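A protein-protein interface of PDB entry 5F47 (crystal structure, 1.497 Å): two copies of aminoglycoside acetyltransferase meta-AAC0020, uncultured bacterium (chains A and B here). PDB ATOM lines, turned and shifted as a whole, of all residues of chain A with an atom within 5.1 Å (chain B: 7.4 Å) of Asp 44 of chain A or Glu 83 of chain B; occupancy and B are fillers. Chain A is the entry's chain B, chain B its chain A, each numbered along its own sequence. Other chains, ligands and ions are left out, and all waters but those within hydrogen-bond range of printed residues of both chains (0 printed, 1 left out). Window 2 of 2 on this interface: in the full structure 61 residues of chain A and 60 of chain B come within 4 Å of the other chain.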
ATOM      1  N   ILE A  42       1.052 -16.710 -33.781  1.00  0.00           N
ATOM      2  CA  ILE A  42       2.101 -16.733 -32.766  1.00  0.00           C
ATOM      3  C   ILE A  42       2.984 -15.482 -32.948  1.00  0.00           C
ATOM      4  O   ILE A  42       3.258 -15.081 -34.066  1.00  0.00           O
ATOM      5  CB  ILE A  42       2.923 -18.052 -32.840  1.00  0.00           C
ATOM      6  CG1 ILE A  42       3.777 -18.220 -31.586  1.00  0.00           C
ATOM      7  CG2 ILE A  42       3.747 -18.138 -34.136  1.00  0.00           C
ATOM      8  CD1 ILE A  42       4.417 -19.607 -31.481  1.00  0.00           C
ATOM      9  N   PRO A  43       3.371 -14.825 -31.836  1.00  0.00           N
ATOM     10  CA  PRO A  43       4.296 -13.688 -31.958  1.00  0.00           C
ATOM     11  C   PRO A  43       5.625 -14.114 -32.562  1.00  0.00           C
ATOM     12  O   PRO A  43       5.917 -15.309 -32.552  1.00  0.00           O
ATOM     13  CB  PRO A  43       4.490 -13.239 -30.507  1.00  0.00           C
ATOM     14  CG  PRO A  43       3.280 -13.708 -29.800  1.00  0.00           C
ATOM     15  CD  PRO A  43       2.888 -14.995 -30.455  1.00  0.00           C
ATOM     16  N   ASP A  44       6.432 -13.182 -33.061  1.00  0.00           N
ATOM     17  CA  ASP A  44       7.682 -13.628 -33.656  1.00  0.00           C
ATOM     18  C   ASP A  44       8.674 -14.048 -32.584  1.00  0.00           C
ATOM     19  O   ASP A  44       8.491 -13.791 -31.382  1.00  0.00           O
ATOM     20  CB  ASP A  44       8.294 -12.573 -34.588  1.00  0.00           C
ATOM     21  CG  ASP A  44       8.835 -11.355 -33.866  1.00  0.00           C
ATOM     22  OD1 ASP A  44       8.692 -11.221 -32.635  1.00  0.00           O
ATOM     23  OD2 ASP A  44       9.419 -10.500 -34.567  1.00  0.00           O
ATOM     24  N   SER A  45       9.705 -14.743 -33.023  1.00  0.00           N
ATOM     25  CA  SER A  45      10.598 -15.412 -32.110  1.00  0.00           C
ATOM     26  C   SER A  45      11.484 -14.438 -31.352  1.00  0.00           C
ATOM     27  O   SER A  45      11.939 -14.744 -30.263  1.00  0.00           O
ATOM     28  CB  SER A  45      11.433 -16.432 -32.871  1.00  0.00           C
ATOM     29  OG  SER A  45      10.596 -17.497 -33.294  1.00  0.00           O
ATOM     30  N   GLU A  46      11.725 -13.265 -31.919  1.00  0.00           N
ATOM     31  CA  GLU A  46      12.449 -12.232 -31.189  1.00  0.00           C
ATOM     32  C   GLU A  46      11.707 -11.876 -29.906  1.00  0.00           C
ATOM     33  O   GLU A  46      12.300 -11.772 -28.828  1.00  0.00           O
ATOM     34  CB  GLU A  46      12.630 -10.993 -32.063  1.00  0.00           C
ATOM     35  CG  GLU A  46      13.241  -9.803 -31.350  1.00  0.00           C
ATOM     36  CD  GLU A  46      13.383  -8.598 -32.264  1.00  0.00           C
ATOM     37  OE1 GLU A  46      13.302  -8.775 -33.500  1.00  0.00           O
ATOM     38  OE2 GLU A  46      13.573  -7.476 -31.749  1.00  0.00           O
ATOM     39  N   HIS A  47      10.395 -11.698 -30.016  1.00  0.00           N
ATOM     40  CA  HIS A  47       9.581 -11.382 -28.853  1.00  0.00           C
ATOM     41  C   HIS A  47       9.566 -12.537 -27.851  1.00  0.00           C
ATOM     42  O   HIS A  47       9.740 -12.346 -26.634  1.00  0.00           O
ATOM     43  CB  HIS A  47       8.142 -11.039 -29.275  1.00  0.00           C
ATOM     44  CG  HIS A  47       7.218 -10.884 -28.107  1.00  0.00           C
ATOM     45  ND1 HIS A  47       7.254  -9.781 -27.285  1.00  0.00           N
ATOM     46  CD2 HIS A  47       6.279 -11.711 -27.593  1.00  0.00           C
ATOM     47  CE1 HIS A  47       6.356  -9.922 -26.326  1.00  0.00           C
ATOM     48  NE2 HIS A  47       5.767 -11.096 -26.473  1.00  0.00           N
ATOM     49  N   LEU A  48       9.355 -13.748 -28.357  1.00  0.00           N
ATOM     50  CA  LEU A  48       9.259 -14.898 -27.473  1.00  0.00           C
ATOM     51  C   LEU A  48      10.592 -15.164 -26.779  1.00  0.00           C
ATOM     52  O   LEU A  48      10.611 -15.554 -25.606  1.00  0.00           O
ATOM     53  CB  LEU A  48       8.794 -16.131 -28.249  1.00  0.00           C
ATOM     54  CG  LEU A  48       7.360 -16.075 -28.785  1.00  0.00           C
ATOM     55  CD1 LEU A  48       7.047 -17.331 -29.584  1.00  0.00           C
ATOM     56  CD2 LEU A  48       6.364 -15.886 -27.637  1.00  0.00           C
ATOM     57  N   GLU B  78       4.159  -9.574 -19.795  1.00  0.00           N
ATOM     58  CA  GLU B  78       4.477  -9.786 -21.197  1.00  0.00           C
ATOM     59  C   GLU B  78       3.923 -11.134 -21.603  1.00  0.00           C
ATOM     60  O   GLU B  78       4.077 -12.121 -20.870  1.00  0.00           O
ATOM     61  CB  GLU B  78       5.983  -9.719 -21.435  1.00  0.00           C
ATOM     62  CG  GLU B  78       6.549  -8.297 -21.387  1.00  0.00           C
ATOM     63  CD  GLU B  78       6.427  -7.493 -22.696  1.00  0.00           C
ATOM     64  OE1 GLU B  78       5.888  -7.962 -23.736  1.00  0.00           O
ATOM     65  OE2 GLU B  78       6.878  -6.336 -22.649  1.00  0.00           O
ATOM     66  N   GLN B  79       3.262 -11.175 -22.751  1.00  0.00           N
ATOM     67  CA  GLN B  79       2.545 -12.375 -23.177  1.00  0.00           C
ATOM     68  C   GLN B  79       3.295 -13.198 -24.196  1.00  0.00           C
ATOM     69  O   GLN B  79       4.133 -12.677 -24.938  1.00  0.00           O
ATOM     70  CB  GLN B  79       1.209 -11.998 -23.811  1.00  0.00           C
ATOM     71  CG  GLN B  79       0.221 -11.305 -22.902  1.00  0.00           C
ATOM     72  CD  GLN B  79      -1.148 -11.299 -23.544  1.00  0.00           C
ATOM     73  OE1 GLN B  79      -1.872 -12.284 -23.473  1.00  0.00           O
ATOM     74  NE2 GLN B  79      -1.492 -10.202 -24.224  1.00  0.00           N
ATOM     75  N   TYR B  80       2.976 -14.482 -24.253  1.00  0.00           N
ATOM     76  CA  TYR B  80       3.441 -15.334 -25.352  1.00  0.00           C
ATOM     77  C   TYR B  80       2.360 -15.516 -26.409  1.00  0.00           C
ATOM     78  O   TYR B  80       2.622 -16.078 -27.460  1.00  0.00           O
ATOM     79  CB  TYR B  80       3.920 -16.709 -24.834  1.00  0.00           C
ATOM     80  CG  TYR B  80       3.070 -17.245 -23.717  1.00  0.00           C
ATOM     81  CD1 TYR B  80       1.987 -18.074 -23.975  1.00  0.00           C
ATOM     82  CD2 TYR B  80       3.343 -16.906 -22.387  1.00  0.00           C
ATOM     83  CE1 TYR B  80       1.187 -18.535 -22.952  1.00  0.00           C
ATOM     84  CE2 TYR B  80       2.548 -17.362 -21.361  1.00  0.00           C
ATOM     85  CZ  TYR B  80       1.486 -18.179 -21.641  1.00  0.00           C
ATOM     86  OH  TYR B  80       0.705 -18.621 -20.604  1.00  0.00           O
ATOM     87  N   TYR B  81       1.151 -15.015 -26.153  1.00  0.00           N
ATOM     88  CA  TYR B  81       0.102 -15.080 -27.181  1.00  0.00           C
ATOM     89  C   TYR B  81       0.084 -13.845 -28.082  1.00  0.00           C
ATOM     90  O   TYR B  81      -0.471 -13.881 -29.183  1.00  0.00           O
ATOM     91  CB  TYR B  81      -1.266 -15.228 -26.544  1.00  0.00           C
ATOM     92  CG  TYR B  81      -1.501 -16.507 -25.759  1.00  0.00           C
ATOM     93  CD1 TYR B  81      -1.156 -17.753 -26.274  1.00  0.00           C
ATOM     94  CD2 TYR B  81      -2.099 -16.453 -24.510  1.00  0.00           C
ATOM     95  CE1 TYR B  81      -1.401 -18.923 -25.551  1.00  0.00           C
ATOM     96  CE2 TYR B  81      -2.337 -17.617 -23.771  1.00  0.00           C
ATOM     97  CZ  TYR B  81      -1.998 -18.838 -24.299  1.00  0.00           C
ATOM     98  OH  TYR B  81      -2.229 -19.993 -23.585  1.00  0.00           O
ATOM     99  N   SER B  82       0.693 -12.767 -27.597  1.00  0.00           N
ATOM    100  CA  SER B  82       0.674 -11.477 -28.291  1.00  0.00           C
ATOM    101  C   SER B  82       1.915 -10.675 -27.923  1.00  0.00           C
ATOM    102  O   SER B  82       2.435 -10.806 -26.814  1.00  0.00           O
ATOM    103  CB  SER B  82      -0.593 -10.696 -27.902  1.00  0.00           C
ATOM    104  OG  SER B  82      -0.656  -9.436 -28.574  1.00  0.00           O
ATOM    105  N   GLU B  83       2.368  -9.804 -28.816  1.00  0.00           N
ATOM    106  CA  GLU B  83       3.414  -8.860 -28.452  1.00  0.00           C
ATOM    107  C   GLU B  83       2.845  -7.700 -27.615  1.00  0.00           C
ATOM    108  O   GLU B  83       3.584  -6.919 -27.041  1.00  0.00           O
ATOM    109  CB  GLU B  83       4.079  -8.327 -29.719  1.00  0.00           C
ATOM    110  CG  GLU B  83       5.438  -7.766 -29.541  1.00  0.00           C
ATOM    111  CD  GLU B  83       6.134  -7.471 -30.882  1.00  0.00           C
ATOM    112  OE1 GLU B  83       6.736  -6.396 -30.992  1.00  0.00           O
ATOM    113  OE2 GLU B  83       6.103  -8.308 -31.809  1.00  0.00           O
ATOM    114  N   LYS B  84       1.517  -7.599 -27.556  1.00  0.00           N
ATOM    115  CA  LYS B  84       0.835  -6.570 -26.756  1.00  0.00           C
ATOM    116  C   LYS B  84       0.637  -7.098 -25.338  1.00  0.00           C
ATOM    117  O   LYS B  84      -0.065  -8.082 -25.166  1.00  0.00           O
ATOM    118  CB  LYS B  84      -0.515  -6.233 -27.392  1.00  0.00           C
ATOM    119  CG  LYS B  84      -0.418  -5.698 -28.821  1.00  0.00           C
ATOM    120  CD  LYS B  84      -1.801  -5.523 -29.441  1.00  0.00           C
ATOM    121  CE  LYS B  84      -1.714  -5.064 -30.905  1.00  0.00           C
ATOM    122  NZ  LYS B  84      -3.057  -4.964 -31.581  1.00  0.00           N
ATOM    123  N   PRO B  85       1.271  -6.468 -24.329  1.00  0.00           N
ATOM    124  CA  PRO B  85       1.214  -7.087 -22.997  1.00  0.00           C
ATOM    125  C   PRO B  85      -0.129  -6.967 -22.298  1.00  0.00           C
ATOM    126  O   PRO B  85      -1.025  -6.233 -22.734  1.00  0.00           O
ATOM    127  CB  PRO B  85       2.269  -6.322 -22.190  1.00  0.00           C
ATOM    128  CG  PRO B  85       3.152  -5.672 -23.211  1.00  0.00           C
ATOM    129  CD  PRO B  85       2.269  -5.385 -24.398  1.00  0.00           C
ATOM    130  N   LEU B  86      -0.247  -7.718 -21.200  1.00  0.00           N
ATOM    131  CA  LEU B  86      -1.348  -7.564 -20.261  1.00  0.00           C
ATOM    132  C   LEU B  86      -0.925  -6.675 -19.109  1.00  0.00           C
ATOM    133  O   LEU B  86       0.244  -6.670 -18.714  1.00  0.00           O
ATOM    134  CB  LEU B  86      -1.791  -8.925 -19.695  1.00  0.00           C
ATOM    135  CG  LEU B  86      -2.281  -9.953 -20.709  1.00  0.00           C
ATOM    136  CD1 LEU B  86      -2.643 -11.235 -19.950  1.00  0.00           C
ATOM    137  CD2 LEU B  86      -3.473  -9.433 -21.498  1.00  0.00           C
ATOM    138  N   LYS B 118       0.414   2.774 -24.318  1.00  0.00           N
ATOM    139  CA  LYS B 118       1.569   1.878 -24.402  1.00  0.00           C
ATOM    140  C   LYS B 118       1.365   0.686 -25.347  1.00  0.00           C
ATOM    141  O   LYS B 118       2.277  -0.127 -25.525  1.00  0.00           O
ATOM    142  CB  LYS B 118       1.923   1.354 -23.011  1.00  0.00           C
ATOM    143  CG  LYS B 118       2.713   2.313 -22.157  1.00  0.00           C
ATOM    144  CD  LYS B 118       3.103   1.641 -20.845  1.00  0.00           C
ATOM    145  CE  LYS B 118       4.268   0.682 -21.001  1.00  0.00           C
ATOM    146  NZ  LYS B 118       5.566   1.395 -21.162  1.00  0.00           N
ATOM    147  N   GLY B 119       0.173   0.551 -25.926  1.00  0.00           N
ATOM    148  CA  GLY B 119      -0.078  -0.545 -26.849  1.00  0.00           C
ATOM    149  C   GLY B 119      -0.295  -1.906 -26.204  1.00  0.00           C
ATOM    150  O   GLY B 119       0.073  -2.950 -26.777  1.00  0.00           O
ATOM    151  N   PHE B 120      -0.888  -1.912 -25.010  1.00  0.00           N
ATOM    152  CA  PHE B 120      -1.255  -3.160 -24.334  1.00  0.00           C
ATOM    153  C   PHE B 120      -2.521  -3.764 -24.931  1.00  0.00           C
ATOM    154  O   PHE B 120      -3.301  -3.083 -25.573  1.00  0.00           O
ATOM    155  CB  PHE B 120      -1.441  -2.920 -22.830  1.00  0.00           C
ATOM    156  CG  PHE B 120      -0.147  -2.918 -22.036  1.00  0.00           C
ATOM    157  CD1 PHE B 120       0.986  -2.239 -22.490  1.00  0.00           C
ATOM    158  CD2 PHE B 120      -0.084  -3.571 -20.816  1.00  0.00           C
ATOM    159  CE1 PHE B 120       2.186  -2.249 -21.723  1.00  0.00           C
ATOM    160  CE2 PHE B 120       1.088  -3.582 -20.048  1.00  0.00           C
ATOM    161  CZ  PHE B 120       2.212  -2.921 -20.482  1.00  0.00           C
ATOM    162  N   GLU B 121      -2.701  -5.065 -24.706  1.00  0.00           N
ATOM    163  CA  GLU B 121      -3.889  -5.762 -25.193  1.00  0.00           C
ATOM    164  C   GLU B 121      -5.085  -5.545 -24.271  1.00  0.00           C
ATOM    165  O   GLU B 121      -6.196  -5.280 -24.722  1.00  0.00           O
ATOM    166  CB  GLU B 121      -3.611  -7.270 -25.322  1.00  0.00           C
ATOM    167  CG  GLU B 121      -4.730  -8.019 -26.026  1.00  0.00           C
ATOM    168  CD  GLU B 121      -4.563  -9.540 -26.032  1.00  0.00           C
ATOM    169  OE1 GLU B 121      -5.066 -10.183 -26.975  1.00  0.00           O
ATOM    170  OE2 GLU B 121      -3.989 -10.096 -25.096  1.00  0.00           O
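The backbone carbonyl oxygen (O) of Gln 79 of chain B sits at hydrogen-bond distance from a ring nitrogen (NE2) of His 47 of chain A (2.7 Å).
A ring nitrogen (NE2) of His 47 of chain A sits at hydrogen-bond distance from the backbone carbonyl oxygen (O) of Ser 82 of chain B.
O of Tyr 80 of chain B touches CD of Pro 43 of chain A, 3.2 Å away.
CG of Pro 43 of chain A touches C of Tyr 81 of chain B, 3.6 Å away.
CG of Pro 43 of chain A touches N of Ser 82 of chain B, 3.5 Å away.
Asp 44 of chain A touches Glu 83 of chain B (OD1 to OE2, 3.98 Å).
OE1 of Glu 78 of chain B touches CE1 of His 47 of chain A, 3.3 Å away.
Glu 83 of chain B touches His 47 of chain A (CG to ND1, 3.5 Å).
CD2 of Leu 48 of chain A touches CA of Tyr 80 of chain B (3.8 Å).
No position is printed for both chains.
Printed residues of chain B that touch a printed residue of chain A: Glu 78, Gln 79, Tyr 80, Tyr 81, Ser 82 and Glu 83.
Hydrophobic or aromatic side chains of chain B that line the printed part of chain A: Tyr 80.
Hydrophobic or aromatic side chains of chain A that line the printed part of chain B: Pro 43, His 47 and Leu 48.
Among the printed residues, 9 pairs touch across the chains.
Among the printed residues, no Asp or Glu carboxylate lies within 4 Å of a Lys or Arg side-chain nitrogen of the other chain.
NE2 of Gln 79 of chain B lies within hydrogen-bond range of O of Lys 84 of chain B (2.7 Å).
OE2 of Glu 121 of chain B sits at hydrogen-bond distance from NE2 of Gln 79 of chain B (2.6 Å).
The side-chain hydroxyl of Ser 82 of chain B is in hydrogen-bond range of the backbone NH of Lys 84 of chain B, at 3.0 Å.
The side-chain carboxylate of Asp 44 of chain A sits at hydrogen-bond distance from the backbone NH of His 47 of chain A, 3.2 Å away.
Of the printed residues of chain B, Asp 44 of chain A touches Glu 83 (3.98 Å).
Of the printed residues of chain A, Glu 83 of chain B touches Asp 44 (3.98 Å) and His 47 (3.5 Å).
Of the printed residues of chain B, Leu 48 of chain A touches Tyr 80.
Printed residues of chain B within 4 Å of Pro 43 of chain A: Tyr 80 (3.2 Å), Tyr 81 (3.6 Å) and Ser 82 (3.5 Å).
Lys 118 of chain B touches none of the printed residues of chain A.
Ile 42 of chain A touches none of the printed residues of chain B.
The nearest printed residue of chain B that does not touch Asp 44 of chain A is Ser 82 of chain B (7.3 Å).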
